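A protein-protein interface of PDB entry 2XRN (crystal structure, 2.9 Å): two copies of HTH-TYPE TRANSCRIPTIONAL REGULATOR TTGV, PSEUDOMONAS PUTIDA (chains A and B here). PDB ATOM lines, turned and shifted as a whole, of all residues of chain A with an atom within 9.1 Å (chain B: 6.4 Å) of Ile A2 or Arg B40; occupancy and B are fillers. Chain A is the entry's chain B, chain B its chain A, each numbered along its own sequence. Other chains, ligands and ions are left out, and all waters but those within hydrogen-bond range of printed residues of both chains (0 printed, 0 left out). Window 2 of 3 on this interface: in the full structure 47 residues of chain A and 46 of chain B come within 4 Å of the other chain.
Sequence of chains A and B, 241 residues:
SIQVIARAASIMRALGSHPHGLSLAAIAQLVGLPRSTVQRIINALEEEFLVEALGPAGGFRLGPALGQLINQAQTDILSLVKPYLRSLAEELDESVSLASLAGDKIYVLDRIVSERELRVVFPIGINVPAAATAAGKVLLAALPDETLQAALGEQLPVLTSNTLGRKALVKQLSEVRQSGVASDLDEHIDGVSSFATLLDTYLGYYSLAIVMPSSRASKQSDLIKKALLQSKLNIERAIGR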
ATOM      1  N   SER A   1      -0.376  30.179  15.199  1.00  0.00           N
ATOM      2  CA  SER A   1      -1.341  29.081  15.228  1.00  0.00           C
ATOM      3  C   SER A   1      -1.086  28.135  14.054  1.00  0.00           C
ATOM      4  O   SER A   1       0.035  27.662  13.880  1.00  0.00           O
ATOM      5  CB  SER A   1      -2.773  29.624  15.195  1.00  0.00           C
ATOM      6  OG  SER A   1      -3.693  28.669  15.695  1.00  0.00           O
ATOM      7  N   ILE A   2      -2.120  27.841  13.265  1.00  0.00           N
ATOM      8  CA  ILE A   2      -1.919  27.161  11.984  1.00  0.00           C
ATOM      9  C   ILE A   2      -2.145  28.134  10.857  1.00  0.00           C
ATOM     10  O   ILE A   2      -3.206  28.742  10.758  1.00  0.00           O
ATOM     11  CB  ILE A   2      -2.897  26.033  11.719  1.00  0.00           C
ATOM     12  CG1 ILE A   2      -2.555  24.798  12.541  1.00  0.00           C
ATOM     13  CG2 ILE A   2      -2.855  25.683  10.247  1.00  0.00           C
ATOM     14  CD1 ILE A   2      -3.370  23.601  12.147  1.00  0.00           C
ATOM     15  N   GLN A   3      -1.157  28.260   9.987  1.00  0.00           N
ATOM     16  CA  GLN A   3      -1.226  29.267   8.953  1.00  0.00           C
ATOM     17  C   GLN A   3      -2.049  28.817   7.754  1.00  0.00           C
ATOM     18  O   GLN A   3      -2.602  29.661   7.044  1.00  0.00           O
ATOM     19  CB  GLN A   3       0.175  29.702   8.521  1.00  0.00           C
ATOM     20  CG  GLN A   3       1.086  30.156   9.670  1.00  0.00           C
ATOM     21  CD  GLN A   3       1.996  29.043  10.199  1.00  0.00           C
ATOM     22  OE1 GLN A   3       3.078  29.309  10.740  1.00  0.00           O
ATOM     23  NE2 GLN A   3       1.561  27.794  10.042  1.00  0.00           N
ATOM     24  N   VAL A   4      -2.164  27.513   7.501  1.00  0.00           N
ATOM     25  CA  VAL A   4      -2.820  27.189   6.238  1.00  0.00           C
ATOM     26  C   VAL A   4      -4.333  27.278   6.345  1.00  0.00           C
ATOM     27  O   VAL A   4      -5.000  27.768   5.434  1.00  0.00           O
ATOM     28  CB  VAL A   4      -2.401  25.860   5.604  1.00  0.00           C
ATOM     29  CG1 VAL A   4      -3.181  24.701   6.203  1.00  0.00           C
ATOM     30  CG2 VAL A   4      -2.661  25.930   4.106  1.00  0.00           C
ATOM     31  N   ILE A   5      -4.868  26.804   7.464  1.00  0.00           N
ATOM     32  CA  ILE A   5      -6.281  26.953   7.740  1.00  0.00           C
ATOM     33  C   ILE A   5      -6.676  28.418   7.661  1.00  0.00           C
ATOM     34  O   ILE A   5      -7.742  28.756   7.149  1.00  0.00           O
ATOM     35  CB  ILE A   5      -6.635  26.394   9.114  1.00  0.00           C
ATOM     36  CG1 ILE A   5      -6.689  24.868   9.042  1.00  0.00           C
ATOM     37  CG2 ILE A   5      -7.967  26.942   9.576  1.00  0.00           C
ATOM     38  CD1 ILE A   5      -6.983  24.206  10.360  1.00  0.00           C
ATOM     39  N   ALA A   6      -5.805  29.287   8.156  1.00  0.00           N
ATOM     40  CA  ALA A   6      -6.056  30.720   8.099  1.00  0.00           C
ATOM     41  C   ALA A   6      -5.995  31.238   6.668  1.00  0.00           C
ATOM     42  O   ALA A   6      -6.745  32.143   6.298  1.00  0.00           O
ATOM     43  CB  ALA A   6      -5.078  31.467   8.982  1.00  0.00           C
ATOM     44  N   ARG A   7      -5.101  30.675   5.861  1.00  0.00           N
ATOM     45  CA  ARG A   7      -5.049  31.054   4.453  1.00  0.00           C
ATOM     46  C   ARG A   7      -6.389  30.708   3.803  1.00  0.00           C
ATOM     47  O   ARG A   7      -7.047  31.560   3.186  1.00  0.00           O
ATOM     48  CB  ARG A   7      -3.881  30.368   3.734  1.00  0.00           C
ATOM     49  CG  ARG A   7      -2.495  30.812   4.221  1.00  0.00           C
ATOM     50  CD  ARG A   7      -1.364  30.351   3.294  1.00  0.00           C
ATOM     51  NE  ARG A   7      -0.806  29.045   3.651  1.00  0.00           N
ATOM     52  CZ  ARG A   7      -0.151  28.251   2.804  1.00  0.00           C
ATOM     53  NH1 ARG A   7       0.016  28.624   1.542  1.00  0.00           N
ATOM     54  NH2 ARG A   7       0.329  27.079   3.211  1.00  0.00           N
ATOM     55  N   ALA A   8      -6.798  29.454   3.973  1.00  0.00           N
ATOM     56  CA  ALA A   8      -8.081  28.977   3.466  1.00  0.00           C
ATOM     57  C   ALA A   8      -9.201  29.927   3.862  1.00  0.00           C
ATOM     58  O   ALA A   8      -9.904  30.469   3.007  1.00  0.00           O
ATOM     59  CB  ALA A   8      -8.366  27.584   3.992  1.00  0.00           C
ATOM     60  N   ALA A   9      -9.353  30.121   5.168  1.00  0.00           N
ATOM     61  CA  ALA A   9     -10.364  31.012   5.719  1.00  0.00           C
ATOM     62  C   ALA A   9     -10.348  32.378   5.052  1.00  0.00           C
ATOM     63  O   ALA A   9     -11.393  32.904   4.696  1.00  0.00           O
ATOM     64  CB  ALA A   9     -10.182  31.155   7.214  1.00  0.00           C
ATOM     65  N   VAL B   4      -5.103  18.742   5.745  1.00  0.00           N
ATOM     66  CA  VAL B   4      -5.587  19.103   7.083  1.00  0.00           C
ATOM     67  C   VAL B   4      -6.848  19.948   6.934  1.00  0.00           C
ATOM     68  O   VAL B   4      -7.719  19.964   7.810  1.00  0.00           O
ATOM     69  CB  VAL B   4      -4.533  19.944   7.849  1.00  0.00           C
ATOM     70  CG1 VAL B   4      -4.398  21.344   7.239  1.00  0.00           C
ATOM     71  CG2 VAL B   4      -4.894  20.051   9.317  1.00  0.00           C
ATOM     72  N   ARG B   7      -9.554  17.767   7.330  1.00  0.00           N
ATOM     73  CA  ARG B   7      -9.820  17.453   8.727  1.00  0.00           C
ATOM     74  C   ARG B   7     -10.699  18.552   9.311  1.00  0.00           C
ATOM     75  O   ARG B   7     -11.773  18.289   9.872  1.00  0.00           O
ATOM     76  CB  ARG B   7      -8.516  17.301   9.520  1.00  0.00           C
ATOM     77  CG  ARG B   7      -7.654  16.108   9.089  1.00  0.00           C
ATOM     78  CD  ARG B   7      -6.533  15.799  10.091  1.00  0.00           C
ATOM     79  NE  ARG B   7      -5.279  16.491   9.792  1.00  0.00           N
ATOM     80  CZ  ARG B   7      -4.325  16.737  10.688  1.00  0.00           C
ATOM     81  NH1 ARG B   7      -4.486  16.361  11.950  1.00  0.00           N
ATOM     82  NH2 ARG B   7      -3.214  17.370  10.329  1.00  0.00           N
ATOM     83  N   ARG B  35      -8.450  13.200  19.932  1.00  0.00           N
ATOM     84  CA  ARG B  35      -8.792  14.373  20.730  1.00  0.00           C
ATOM     85  C   ARG B  35      -7.741  15.481  20.611  1.00  0.00           C
ATOM     86  O   ARG B  35      -8.080  16.664  20.556  1.00  0.00           O
ATOM     87  CB  ARG B  35      -8.929  13.929  22.187  1.00  0.00           C
ATOM     88  CG  ARG B  35      -9.241  15.033  23.178  1.00  0.00           C
ATOM     89  CD  ARG B  35      -9.239  14.484  24.593  1.00  0.00           C
ATOM     90  NE  ARG B  35      -9.956  13.213  24.671  1.00  0.00           N
ATOM     91  CZ  ARG B  35     -11.201  13.084  25.115  1.00  0.00           C
ATOM     92  NH1 ARG B  35     -11.869  14.150  25.533  1.00  0.00           N
ATOM     93  NH2 ARG B  35     -11.776  11.889  25.148  1.00  0.00           N
ATOM     94  N   SER B  36      -6.471  15.089  20.569  1.00  0.00           N
ATOM     95  CA  SER B  36      -5.364  16.037  20.470  1.00  0.00           C
ATOM     96  C   SER B  36      -5.370  16.855  19.176  1.00  0.00           C
ATOM     97  O   SER B  36      -5.591  18.072  19.198  1.00  0.00           O
ATOM     98  CB  SER B  36      -4.027  15.310  20.613  1.00  0.00           C
ATOM     99  OG  SER B  36      -2.947  16.155  20.253  1.00  0.00           O
ATOM    100  N   THR B  37      -5.115  16.195  18.051  1.00  0.00           N
ATOM    101  CA  THR B  37      -5.014  16.908  16.779  1.00  0.00           C
ATOM    102  C   THR B  37      -6.298  17.702  16.500  1.00  0.00           C
ATOM    103  O   THR B  37      -6.267  18.782  15.889  1.00  0.00           O
ATOM    104  CB  THR B  37      -4.674  15.959  15.610  1.00  0.00           C
ATOM    105  OG1 THR B  37      -5.829  15.766  14.787  1.00  0.00           O
ATOM    106  CG2 THR B  37      -4.192  14.614  16.136  1.00  0.00           C
ATOM    107  N   VAL B  38      -7.422  17.169  16.972  1.00  0.00           N
ATOM    108  CA  VAL B  38      -8.689  17.883  16.905  1.00  0.00           C
ATOM    109  C   VAL B  38      -8.585  19.189  17.673  1.00  0.00           C
ATOM    110  O   VAL B  38      -8.803  20.254  17.115  1.00  0.00           O
ATOM    111  CB  VAL B  38      -9.847  17.059  17.468  1.00  0.00           C
ATOM    112  CG1 VAL B  38     -11.047  17.952  17.704  1.00  0.00           C
ATOM    113  CG2 VAL B  38     -10.195  15.930  16.519  1.00  0.00           C
ATOM    114  N   GLN B  39      -8.246  19.107  18.955  1.00  0.00           N
ATOM    115  CA  GLN B  39      -7.995  20.310  19.740  1.00  0.00           C
ATOM    116  C   GLN B  39      -7.174  21.322  18.935  1.00  0.00           C
ATOM    117  O   GLN B  39      -7.519  22.504  18.858  1.00  0.00           O
ATOM    118  CB  GLN B  39      -7.279  19.949  21.043  1.00  0.00           C
ATOM    119  CG  GLN B  39      -6.928  21.140  21.909  1.00  0.00           C
ATOM    120  CD  GLN B  39      -8.149  21.814  22.485  1.00  0.00           C
ATOM    121  OE1 GLN B  39      -9.007  21.164  23.085  1.00  0.00           O
ATOM    122  NE2 GLN B  39      -8.240  23.124  22.298  1.00  0.00           N
ATOM    123  N   ARG B  40      -6.094  20.847  18.326  1.00  0.00           N
ATOM    124  CA  ARG B  40      -5.247  21.696  17.499  1.00  0.00           C
ATOM    125  C   ARG B  40      -6.086  22.445  16.470  1.00  0.00           C
ATOM    126  O   ARG B  40      -6.077  23.686  16.405  1.00  0.00           O
ATOM    127  CB  ARG B  40      -4.199  20.839  16.776  1.00  0.00           C
ATOM    128  CG  ARG B  40      -2.934  21.579  16.333  1.00  0.00           C
ATOM    129  CD  ARG B  40      -2.625  21.392  14.835  1.00  0.00           C
ATOM    130  NE  ARG B  40      -2.908  20.042  14.338  1.00  0.00           N
ATOM    131  CZ  ARG B  40      -2.456  19.550  13.184  1.00  0.00           C
ATOM    132  NH1 ARG B  40      -1.675  20.286  12.397  1.00  0.00           N
ATOM    133  NH2 ARG B  40      -2.781  18.312  12.816  1.00  0.00           N
ATOM    134  N   ILE B  41      -6.817  21.679  15.665  1.00  0.00           N
ATOM    135  CA  ILE B  41      -7.576  22.247  14.552  1.00  0.00           C
ATOM    136  C   ILE B  41      -8.666  23.210  15.016  1.00  0.00           C
ATOM    137  O   ILE B  41      -8.813  24.309  14.476  1.00  0.00           O
ATOM    138  CB  ILE B  41      -8.199  21.154  13.685  1.00  0.00           C
ATOM    139  CG1 ILE B  41      -7.098  20.237  13.144  1.00  0.00           C
ATOM    140  CG2 ILE B  41      -8.997  21.781  12.553  1.00  0.00           C
ATOM    141  CD1 ILE B  41      -7.565  18.837  12.844  1.00  0.00           C
ATOM    142  N   ILE B  42      -9.434  22.788  16.012  1.00  0.00           N
ATOM    143  CA  ILE B  42     -10.373  23.681  16.655  1.00  0.00           C
ATOM    144  C   ILE B  42      -9.663  24.996  16.908  1.00  0.00           C
ATOM    145  O   ILE B  42     -10.047  26.007  16.353  1.00  0.00           O
ATOM    146  CB  ILE B  42     -10.892  23.123  17.975  1.00  0.00           C
ATOM    147  CG1 ILE B  42     -11.769  21.898  17.724  1.00  0.00           C
ATOM    148  CG2 ILE B  42     -11.700  24.174  18.697  1.00  0.00           C
ATOM    149  CD1 ILE B  42     -13.040  22.209  16.978  1.00  0.00           C
ATOM    150  N   ASN B  43      -8.610  24.983  17.719  1.00  0.00           N
ATOM    151  CA  ASN B  43      -7.861  26.215  17.980  1.00  0.00           C
ATOM    152  C   ASN B  43      -7.629  27.043  16.717  1.00  0.00           C
ATOM    153  O   ASN B  43      -7.859  28.260  16.704  1.00  0.00           O
ATOM    154  CB  ASN B  43      -6.528  25.916  18.667  1.00  0.00           C
ATOM    155  CG  ASN B  43      -6.705  25.390  20.074  1.00  0.00           C
ATOM    156  OD1 ASN B  43      -7.808  25.024  20.481  1.00  0.00           O
ATOM    157  ND2 ASN B  43      -5.616  25.344  20.826  1.00  0.00           N
ATOM    158  N   ALA B  44      -7.181  26.377  15.655  1.00  0.00           N
ATOM    159  CA  ALA B  44      -6.922  27.069  14.391  1.00  0.00           C
ATOM    160  C   ALA B  44      -8.162  27.799  13.871  1.00  0.00           C
ATOM    161  O   ALA B  44      -8.084  28.946  13.412  1.00  0.00           O
ATOM    162  CB  ALA B  44      -6.417  26.088  13.347  1.00  0.00           C
ATOM    163  N   LEU B  45      -9.301  27.115  13.940  1.00  0.00           N
ATOM    164  CA  LEU B  45     -10.563  27.659  13.461  1.00  0.00           C
ATOM    165  C   LEU B  45     -11.024  28.808  14.347  1.00  0.00           C
ATOM    166  O   LEU B  45     -11.431  29.863  13.860  1.00  0.00           O
ATOM    167  CB  LEU B  45     -11.624  26.559  13.424  1.00  0.00           C
ATOM    168  CG  LEU B  45     -11.315  25.394  12.475  1.00  0.00           C
ATOM    169  CD1 LEU B  45     -12.250  24.215  12.708  1.00  0.00           C
ATOM    170  CD2 LEU B  45     -11.380  25.853  11.032  1.00  0.00           C
ATOM    171  N   GLU B  48     -10.077  32.074  13.816  1.00  0.00           N
ATOM    172  CA  GLU B  48     -10.726  32.677  12.656  1.00  0.00           C
ATOM    173  C   GLU B  48     -12.205  32.964  12.888  1.00  0.00           C
ATOM    174  O   GLU B  48     -12.908  33.416  11.984  1.00  0.00           O
ATOM    175  CB  GLU B  48     -10.559  31.784  11.423  1.00  0.00           C
ATOM    176  CG  GLU B  48      -9.137  31.671  10.916  1.00  0.00           C
ATOM    177  CD  GLU B  48      -8.547  33.008  10.523  1.00  0.00           C
ATOM    178  OE1 GLU B  48      -8.890  34.027  11.159  1.00  0.00           O
ATOM    179  OE2 GLU B  48      -7.739  33.041   9.571  1.00  0.00           O
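The guanidinium group (NH2) of Arg B40 sits close to the guanidinium group (NH2) of Arg B7 (2.7 Å).
Among the printed residues, pairs that only touch across the chains: Ser A1 with Ala B44 (3.8 Å), Ile A2 with Arg B40 (3.6 Å), Ile A2 with Ala B44 (3.9 Å), Val A4 with Val B4 (3.7 Å), Ile A5 with Ile B41 (3.8 Å), Ile A5 with Ala B44 (3.6 Å), Ile A5 with Leu B45 (3.9 Å), Ala A6 with Glu B48 (3.1 Å) and Ala A9 with Glu B48 (3.9 Å).
Of chain B, only Arg B40 and Ala B44 come within 4 Å of Ile A2.
Arg B40 touches just one residue of chain A: Ile A2.
Ile B41 touches just one residue of chain A: Ile A5 (3.8 Å).
No residue of chain A comes within 4 Å of Asn B43.
Of the printed residues of chain A, Val B4 touches Val A4.
Of the printed residues of chain A, Ala B44 touches Ser A1, Ile A2 and Ile A5.
Printed residues of chain A within 4 Å of Glu B48: Ala A6 (3.1 Å) and Ala A9 (3.9 Å).
Printed residues of chain B within 4 Å of Ala A9: Glu B48.
Printed residues of chain B within 4 Å of Val A4: Val B4.
Arg B35 touches none of the printed residues of chain A.
Ala A8 touches none of the printed residues of chain B.
The nearest residue of chain B that does not touch Ile A2 is Val B4 (4.8 Å).
Printed residues of chain B that touch a printed residue of chain A: Val B4, Arg B40, Ile B41, Ala B44, Leu B45 and Glu B48.
Hydrophobic or aromatic side chains of chain B that line the printed part of chain A: Val B4, Ile B41, Ala B44 and Leu B45.
Hydrophobic or aromatic side chains of chain A within 4 Å of the printed part of chain B: Ile A2, Val A4, Ile A5, Ala A6 and Ala A9.
Val B4 touches its own counterpart, Val A4.
Of the 9 pairs that touch across the chains among the printed residues, 1 has its exchanged pair printed and touching as well.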
